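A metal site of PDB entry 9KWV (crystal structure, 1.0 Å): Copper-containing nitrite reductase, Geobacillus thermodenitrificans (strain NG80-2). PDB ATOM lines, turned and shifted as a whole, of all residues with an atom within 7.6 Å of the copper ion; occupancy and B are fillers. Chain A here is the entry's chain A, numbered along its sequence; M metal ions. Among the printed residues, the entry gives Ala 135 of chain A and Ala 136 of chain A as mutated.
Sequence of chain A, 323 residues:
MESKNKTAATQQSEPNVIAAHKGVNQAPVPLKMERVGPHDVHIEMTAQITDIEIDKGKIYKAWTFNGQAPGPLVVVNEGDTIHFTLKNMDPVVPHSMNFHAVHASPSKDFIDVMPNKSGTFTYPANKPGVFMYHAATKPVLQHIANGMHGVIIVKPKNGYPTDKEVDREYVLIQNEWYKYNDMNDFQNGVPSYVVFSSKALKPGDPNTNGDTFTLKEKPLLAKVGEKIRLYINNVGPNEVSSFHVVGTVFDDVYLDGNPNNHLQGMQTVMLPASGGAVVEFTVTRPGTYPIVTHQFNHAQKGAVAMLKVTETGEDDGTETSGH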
ATOM      1  N   ALA A  47       7.995   9.995  -5.278  1.00  0.00           N
ATOM      2  CA  ALA A  47       9.382  10.437  -5.153  1.00  0.00           C
ATOM      3  C   ALA A  47       9.351  11.703  -4.314  1.00  0.00           C
ATOM      4  O   ALA A  47       8.612  12.645  -4.638  1.00  0.00           O
ATOM      5  CB  ALA A  47       9.999  10.717  -6.525  1.00  0.00           C
ATOM      6  N   GLN A  48      10.104  11.731  -3.223  1.00  0.00           N
ATOM      7  CA  GLN A  48      10.016  12.846  -2.294  1.00  0.00           C
ATOM      8  C   GLN A  48      11.324  13.006  -1.526  1.00  0.00           C
ATOM      9  O   GLN A  48      12.139  12.075  -1.441  1.00  0.00           O
ATOM     10  CB  GLN A  48       8.816  12.671  -1.346  1.00  0.00           C
ATOM     11  CG  GLN A  48       8.901  11.437  -0.458  1.00  0.00           C
ATOM     12  CD  GLN A  48       7.683  11.331   0.429  1.00  0.00           C
ATOM     13  OE1 GLN A  48       6.628  10.842   0.023  1.00  0.00           O
ATOM     14  NE2 GLN A  48       7.795  11.839   1.635  1.00  0.00           N
ATOM     15  N   ILE A  49      11.506  14.201  -0.990  1.00  0.00           N
ATOM     16  CA  ILE A  49      12.731  14.635  -0.330  1.00  0.00           C
ATOM     17  C   ILE A  49      12.465  14.659   1.166  1.00  0.00           C
ATOM     18  O   ILE A  49      11.619  15.440   1.630  1.00  0.00           O
ATOM     19  CB  ILE A  49      13.141  16.021  -0.853  1.00  0.00           C
ATOM     20  CG1 ILE A  49      13.323  16.017  -2.395  1.00  0.00           C
ATOM     21  CG2 ILE A  49      14.391  16.522  -0.135  1.00  0.00           C
ATOM     22  CD1 ILE A  49      14.321  14.980  -2.903  1.00  0.00           C
ATOM     23  N   TRP A  63      16.889  11.525  -1.125  1.00  0.00           N
ATOM     24  CA  TRP A  63      16.009  11.358  -2.270  1.00  0.00           C
ATOM     25  C   TRP A  63      15.368   9.993  -2.118  1.00  0.00           C
ATOM     26  O   TRP A  63      16.065   8.982  -2.114  1.00  0.00           O
ATOM     27  CB  TRP A  63      16.807  11.420  -3.563  1.00  0.00           C
ATOM     28  CG  TRP A  63      17.542  12.708  -3.856  1.00  0.00           C
ATOM     29  CD1 TRP A  63      17.729  13.790  -3.028  1.00  0.00           C
ATOM     30  CD2 TRP A  63      18.206  13.022  -5.077  1.00  0.00           C
ATOM     31  NE1 TRP A  63      18.460  14.755  -3.688  1.00  0.00           N
ATOM     32  CE2 TRP A  63      18.760  14.303  -4.946  1.00  0.00           C
ATOM     33  CE3 TRP A  63      18.396  12.327  -6.275  1.00  0.00           C
ATOM     34  CZ2 TRP A  63      19.502  14.903  -5.968  1.00  0.00           C
ATOM     35  CZ3 TRP A  63      19.125  12.920  -7.287  1.00  0.00           C
ATOM     36  CH2 TRP A  63      19.660  14.194  -7.135  1.00  0.00           C
ATOM     37  N   THR A  64      14.038   9.952  -1.943  1.00  0.00           N
ATOM     38  CA  THR A  64      13.373   8.742  -1.490  1.00  0.00           C
ATOM     39  C   THR A  64      12.154   8.400  -2.324  1.00  0.00           C
ATOM     40  O   THR A  64      11.542   9.252  -2.976  1.00  0.00           O
ATOM     41  CB  THR A  64      12.879   8.840  -0.036  1.00  0.00           C
ATOM     42  OG1 THR A  64      11.706   9.658   0.055  1.00  0.00           O
ATOM     43  CG2 THR A  64      13.955   9.376   0.896  1.00  0.00           C
ATOM     44  N   PHE A  65      11.795   7.120  -2.250  1.00  0.00           N
ATOM     45  CA  PHE A  65      10.442   6.668  -2.519  1.00  0.00           C
ATOM     46  C   PHE A  65       9.664   6.684  -1.206  1.00  0.00           C
ATOM     47  O   PHE A  65      10.041   6.015  -0.235  1.00  0.00           O
ATOM     48  CB  PHE A  65      10.455   5.283  -3.138  1.00  0.00           C
ATOM     49  CG  PHE A  65      11.177   5.209  -4.471  1.00  0.00           C
ATOM     50  CD1 PHE A  65      10.631   5.806  -5.597  1.00  0.00           C
ATOM     51  CD2 PHE A  65      12.403   4.588  -4.584  1.00  0.00           C
ATOM     52  CE1 PHE A  65      11.278   5.749  -6.819  1.00  0.00           C
ATOM     53  CE2 PHE A  65      13.052   4.521  -5.821  1.00  0.00           C
ATOM     54  CZ  PHE A  65      12.496   5.107  -6.927  1.00  0.00           C
ATOM     55  N   LEU A  86       4.238   6.485 -10.399  1.00  0.00           N
ATOM     56  CA  LEU A  86       5.128   7.313  -9.607  1.00  0.00           C
ATOM     57  C   LEU A  86       4.624   8.747  -9.640  1.00  0.00           C
ATOM     58  O   LEU A  86       4.451   9.330 -10.717  1.00  0.00           O
ATOM     59  CB  LEU A  86       6.566   7.274 -10.157  1.00  0.00           C
ATOM     60  CG  LEU A  86       7.618   8.045  -9.342  1.00  0.00           C
ATOM     61  CD1 LEU A  86       7.813   7.440  -7.949  1.00  0.00           C
ATOM     62  CD2 LEU A  86       8.934   8.079 -10.085  1.00  0.00           C
ATOM     63  N   ASN A  88       5.773  12.354  -8.605  1.00  0.00           N
ATOM     64  CA  ASN A  88       7.014  13.059  -8.267  1.00  0.00           C
ATOM     65  C   ASN A  88       6.694  14.334  -7.500  1.00  0.00           C
ATOM     66  O   ASN A  88       6.195  15.304  -8.070  1.00  0.00           O
ATOM     67  CB  ASN A  88       7.842  13.372  -9.512  1.00  0.00           C
ATOM     68  CG  ASN A  88       9.204  13.917  -9.164  1.00  0.00           C
ATOM     69  OD1 ASN A  88       9.538  14.070  -7.988  1.00  0.00           O
ATOM     70  ND2 ASN A  88      10.000  14.219 -10.176  1.00  0.00           N
ATOM     71  N   ASP A  90       9.142  15.969  -5.817  1.00  0.00           N
ATOM     72  CA  ASP A  90      10.343  16.799  -5.795  1.00  0.00           C
ATOM     73  C   ASP A  90      10.058  18.063  -6.593  1.00  0.00           C
ATOM     74  O   ASP A  90       9.545  17.982  -7.712  1.00  0.00           O
ATOM     75  CB  ASP A  90      11.482  15.993  -6.434  1.00  0.00           C
ATOM     76  CG  ASP A  90      12.858  16.646  -6.299  1.00  0.00           C
ATOM     77  OD1 ASP A  90      12.961  17.878  -6.477  1.00  0.00           O
ATOM     78  OD2 ASP A  90      13.837  15.890  -6.091  1.00  0.00           O
ATOM     79  N   VAL A  93      13.842  18.051  -9.327  1.00  0.00           N
ATOM     80  CA  VAL A  93      14.586  16.936  -9.917  1.00  0.00           C
ATOM     81  C   VAL A  93      13.618  15.902 -10.474  1.00  0.00           C
ATOM     82  O   VAL A  93      12.718  15.451  -9.744  1.00  0.00           O
ATOM     83  CB  VAL A  93      15.564  16.284  -8.910  1.00  0.00           C
ATOM     84  CG1 VAL A  93      16.426  15.248  -9.620  1.00  0.00           C
ATOM     85  CG2 VAL A  93      16.431  17.323  -8.232  1.00  0.00           C
ATOM     86  N   PRO A  94      13.788  15.462 -11.732  1.00  0.00           N
ATOM     87  CA  PRO A  94      13.019  14.306 -12.226  1.00  0.00           C
ATOM     88  C   PRO A  94      13.455  13.027 -11.517  1.00  0.00           C
ATOM     89  O   PRO A  94      14.610  12.885 -11.111  1.00  0.00           O
ATOM     90  CB  PRO A  94      13.386  14.250 -13.714  1.00  0.00           C
ATOM     91  CG  PRO A  94      13.945  15.593 -14.040  1.00  0.00           C
ATOM     92  CD  PRO A  94      14.656  16.012 -12.786  1.00  0.00           C
ATOM     93  N   HIS A  95      12.531  12.079 -11.413  1.00  0.00           N
ATOM     94  CA  HIS A  95      12.827  10.752 -10.878  1.00  0.00           C
ATOM     95  C   HIS A  95      12.114   9.700 -11.718  1.00  0.00           C
ATOM     96  O   HIS A  95      11.357  10.017 -12.633  1.00  0.00           O
ATOM     97  CB  HIS A  95      12.454  10.648  -9.383  1.00  0.00           C
ATOM     98  CG  HIS A  95      13.144  11.661  -8.520  1.00  0.00           C
ATOM     99  ND1 HIS A  95      14.472  11.573  -8.154  1.00  0.00           N
ATOM    100  CD2 HIS A  95      12.677  12.811  -7.979  1.00  0.00           C
ATOM    101  CE1 HIS A  95      14.783  12.631  -7.413  1.00  0.00           C
ATOM    102  NE2 HIS A  95      13.709  13.403  -7.298  1.00  0.00           N
ATOM    103  N   SER A  96      12.374   8.423 -11.436  1.00  0.00           N
ATOM    104  CA  SER A  96      11.894   7.324 -12.259  1.00  0.00           C
ATOM    105  C   SER A  96      12.037   6.041 -11.447  1.00  0.00           C
ATOM    106  O   SER A  96      12.543   6.053 -10.316  1.00  0.00           O
ATOM    107  CB  SER A  96      12.714   7.211 -13.544  1.00  0.00           C
ATOM    108  OG  SER A  96      14.079   6.940 -13.226  1.00  0.00           O
ATOM    109  N   HIS A 134      15.103   0.691  -7.982  1.00  0.00           N
ATOM    110  CA  HIS A 134      15.841   1.940  -7.792  1.00  0.00           C
ATOM    111  C   HIS A 134      15.446   2.915  -8.901  1.00  0.00           C
ATOM    112  O   HIS A 134      14.874   2.532  -9.922  1.00  0.00           O
ATOM    113  CB  HIS A 134      17.360   1.705  -7.802  1.00  0.00           C
ATOM    114  CG  HIS A 134      17.865   1.085  -9.064  1.00  0.00           C
ATOM    115  ND1 HIS A 134      18.180   1.831 -10.183  1.00  0.00           N
ATOM    116  CD2 HIS A 134      18.156  -0.202  -9.389  1.00  0.00           C
ATOM    117  CE1 HIS A 134      18.635   1.021 -11.137  1.00  0.00           C
ATOM    118  NE2 HIS A 134      18.650  -0.210 -10.670  1.00  0.00           N
ATOM    119  N   ALA A 135      15.806   4.182  -8.706  1.00  0.00           N
ATOM    120  CA  ALA A 135      15.570   5.152  -9.765  1.00  0.00           C
ATOM    121  C   ALA A 135      16.495   4.915 -10.954  1.00  0.00           C
ATOM    122  O   ALA A 135      17.628   4.449 -10.808  1.00  0.00           O
ATOM    123  CB  ALA A 135      15.735   6.577  -9.233  1.00  0.00           C
ATOM    124  N   ALA A 136      16.011   5.274 -12.147  1.00  0.00           N
ATOM    125  CA  ALA A 136      16.714   5.045 -13.407  1.00  0.00           C
ATOM    126  C   ALA A 136      17.198   6.325 -14.056  1.00  0.00           C
ATOM    127  O   ALA A 136      17.737   6.292 -15.172  1.00  0.00           O
ATOM    128  CB  ALA A 136      15.840   4.234 -14.375  1.00  0.00           C
ATOM    129  N   THR A 137      17.100   7.441 -13.367  1.00  0.00           N
ATOM    130  CA  THR A 137      17.375   8.756 -13.924  1.00  0.00           C
ATOM    131  C   THR A 137      18.868   9.023 -13.897  1.00  0.00           C
ATOM    132  O   THR A 137      19.534   8.812 -12.875  1.00  0.00           O
ATOM    133  CB  THR A 137      16.616   9.788 -13.082  1.00  0.00           C
ATOM    134  OG1 THR A 137      15.206   9.497 -13.096  1.00  0.00           O
ATOM    135  CG2 THR A 137      16.850  11.214 -13.569  1.00  0.00           C
ATOM    136  N   PRO A 139      22.295  10.965 -13.482  1.00  0.00           N
ATOM    137  CA  PRO A 139      23.189   9.820 -13.240  1.00  0.00           C
ATOM    138  C   PRO A 139      22.579   8.873 -12.223  1.00  0.00           C
ATOM    139  O   PRO A 139      22.233   9.289 -11.106  1.00  0.00           O
ATOM    140  CB  PRO A 139      24.460  10.467 -12.660  1.00  0.00           C
ATOM    141  CG  PRO A 139      24.245  11.929 -12.684  1.00  0.00           C
ATOM    142  CD  PRO A 139      22.765  12.167 -12.785  1.00  0.00           C
ATOM    143  N   VAL A 140      22.462   7.595 -12.593  1.00  0.00           N
ATOM    144  CA  VAL A 140      21.828   6.634 -11.714  1.00  0.00           C
ATOM    145  C   VAL A 140      22.575   6.532 -10.386  1.00  0.00           C
ATOM    146  O   VAL A 140      21.960   6.409  -9.316  1.00  0.00           O
ATOM    147  CB  VAL A 140      21.670   5.279 -12.426  1.00  0.00           C
ATOM    148  CG1 VAL A 140      21.238   4.194 -11.475  1.00  0.00           C
ATOM    149  CG2 VAL A 140      20.650   5.417 -13.567  1.00  0.00           C
ATOM    150  N   GLN A 142      23.940   8.841  -8.701  1.00  0.00           N
ATOM    151  CA  GLN A 142      23.506   9.934  -7.824  1.00  0.00           C
ATOM    152  C   GLN A 142      22.171   9.614  -7.152  1.00  0.00           C
ATOM    153  O   GLN A 142      21.984   9.856  -5.950  1.00  0.00           O
ATOM    154  CB  GLN A 142      23.399  11.222  -8.640  1.00  0.00           C
ATOM    155  CG  GLN A 142      23.153  12.462  -7.788  1.00  0.00           C
ATOM    156  CD  GLN A 142      23.202  13.732  -8.589  1.00  0.00           C
ATOM    157  OE1 GLN A 142      23.139  13.722  -9.814  1.00  0.00           O
ATOM    158  NE2 GLN A 142      23.311  14.851  -7.897  1.00  0.00           N
ATOM    159  N   HIS A 143      21.220   9.081  -7.932  1.00  0.00           N
ATOM    160  CA  HIS A 143      19.910   8.762  -7.379  1.00  0.00           C
ATOM    161  C   HIS A 143      19.977   7.617  -6.378  1.00  0.00           C
ATOM    162  O   HIS A 143      19.339   7.694  -5.320  1.00  0.00           O
ATOM    163  CB  HIS A 143      18.904   8.459  -8.494  1.00  0.00           C
ATOM    164  CG  HIS A 143      18.501   9.677  -9.268  1.00  0.00           C
ATOM    165  ND1 HIS A 143      17.288  10.312  -9.089  1.00  0.00           N
ATOM    166  CD2 HIS A 143      19.194  10.415 -10.168  1.00  0.00           C
ATOM    167  CE1 HIS A 143      17.251  11.371  -9.877  1.00  0.00           C
ATOM    168  NE2 HIS A 143      18.397  11.456 -10.539  1.00  0.00           N
ATOM    169  N   ILE A 144      20.731   6.553  -6.692  1.00  0.00           N
ATOM    170  CA  ILE A 144      20.854   5.458  -5.738  1.00  0.00           C
ATOM    171  C   ILE A 144      21.549   5.928  -4.467  1.00  0.00           C
ATOM    172  O   ILE A 144      21.081   5.704  -3.352  1.00  0.00           O
ATOM    173  CB  ILE A 144      21.574   4.236  -6.356  1.00  0.00           C
ATOM    174  CG1 ILE A 144      20.798   3.680  -7.568  1.00  0.00           C
ATOM    175  CG2 ILE A 144      21.743   3.151  -5.300  1.00  0.00           C
ATOM    176  CD1 ILE A 144      21.510   2.538  -8.266  1.00  0.00           C
ATOM    177  N   ASN A 146      21.820   8.784  -3.129  1.00  0.00           N
ATOM    178  CA  ASN A 146      21.018   9.698  -2.326  1.00  0.00           C
ATOM    179  C   ASN A 146      19.803   9.041  -1.676  1.00  0.00           C
ATOM    180  O   ASN A 146      19.121   9.707  -0.879  1.00  0.00           O
ATOM    181  CB  ASN A 146      20.577  10.913  -3.148  1.00  0.00           C
ATOM    182  CG  ASN A 146      21.676  11.953  -3.313  1.00  0.00           C
ATOM    183  OD1 ASN A 146      22.531  12.139  -2.453  1.00  0.00           O
ATOM    184  ND2 ASN A 146      21.626  12.675  -4.429  1.00  0.00           N
ATOM    185  N   GLY A 147      19.518   7.763  -1.948  1.00  0.00           N
ATOM    186  CA  GLY A 147      18.499   7.019  -1.225  1.00  0.00           C
ATOM    187  C   GLY A 147      17.453   6.295  -2.058  1.00  0.00           C
ATOM    188  O   GLY A 147      16.596   5.630  -1.460  1.00  0.00           O
ATOM    189  N   MET A 148      17.477   6.388  -3.391  1.00  0.00           N
ATOM    190  CA  MET A 148      16.375   5.877  -4.217  1.00  0.00           C
ATOM    191  C   MET A 148      16.663   4.433  -4.609  1.00  0.00           C
ATOM    192  O   MET A 148      17.004   4.096  -5.755  1.00  0.00           O
ATOM    193  CB  MET A 148      16.192   6.784  -5.429  1.00  0.00           C
ATOM    194  CG  MET A 148      15.496   8.050  -5.127  1.00  0.00           C
ATOM    195  SD  MET A 148      14.592   8.743  -6.552  1.00  0.00           S
ATOM    196  CE  MET A 148      13.450   9.708  -5.624  1.00  0.00           C
HETATM  197 CU    CU M   1      15.735   9.925  -7.943  1.00  0.00          CU
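The backbone NH of Ala 135 sits at hydrogen-bond distance from the backbone carbonyl oxygen of Met 148 (3.2 Å).
The backbone NH (N) of Met 148 lies close to the backbone carbonyl oxygen (O) of Trp 63 (3.2 Å).
NE2 of His 95 lies close to O of Val 93, 3.3 Å away.
A ring nitrogen (NE2) of His 95 sits at hydrogen-bond distance from the side-chain carboxylate (OD2) of Asp 90.
N of Trp 63 sits at hydrogen-bond distance from O of Asn 146, 2.9 Å away.
Trp 63 touches the copper ion (CE3 to CU, 3.95 Å).
CB of Ala 135 touches the copper ion, 3.6 Å away.
The copper ion is bound by a ring nitrogen (ND1) of His 143 (2.0 Å), a ring nitrogen (ND1) of His 95 (2.1 Å) and the side-chain sulfur (SD) of Met 148 (2.2 Å).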
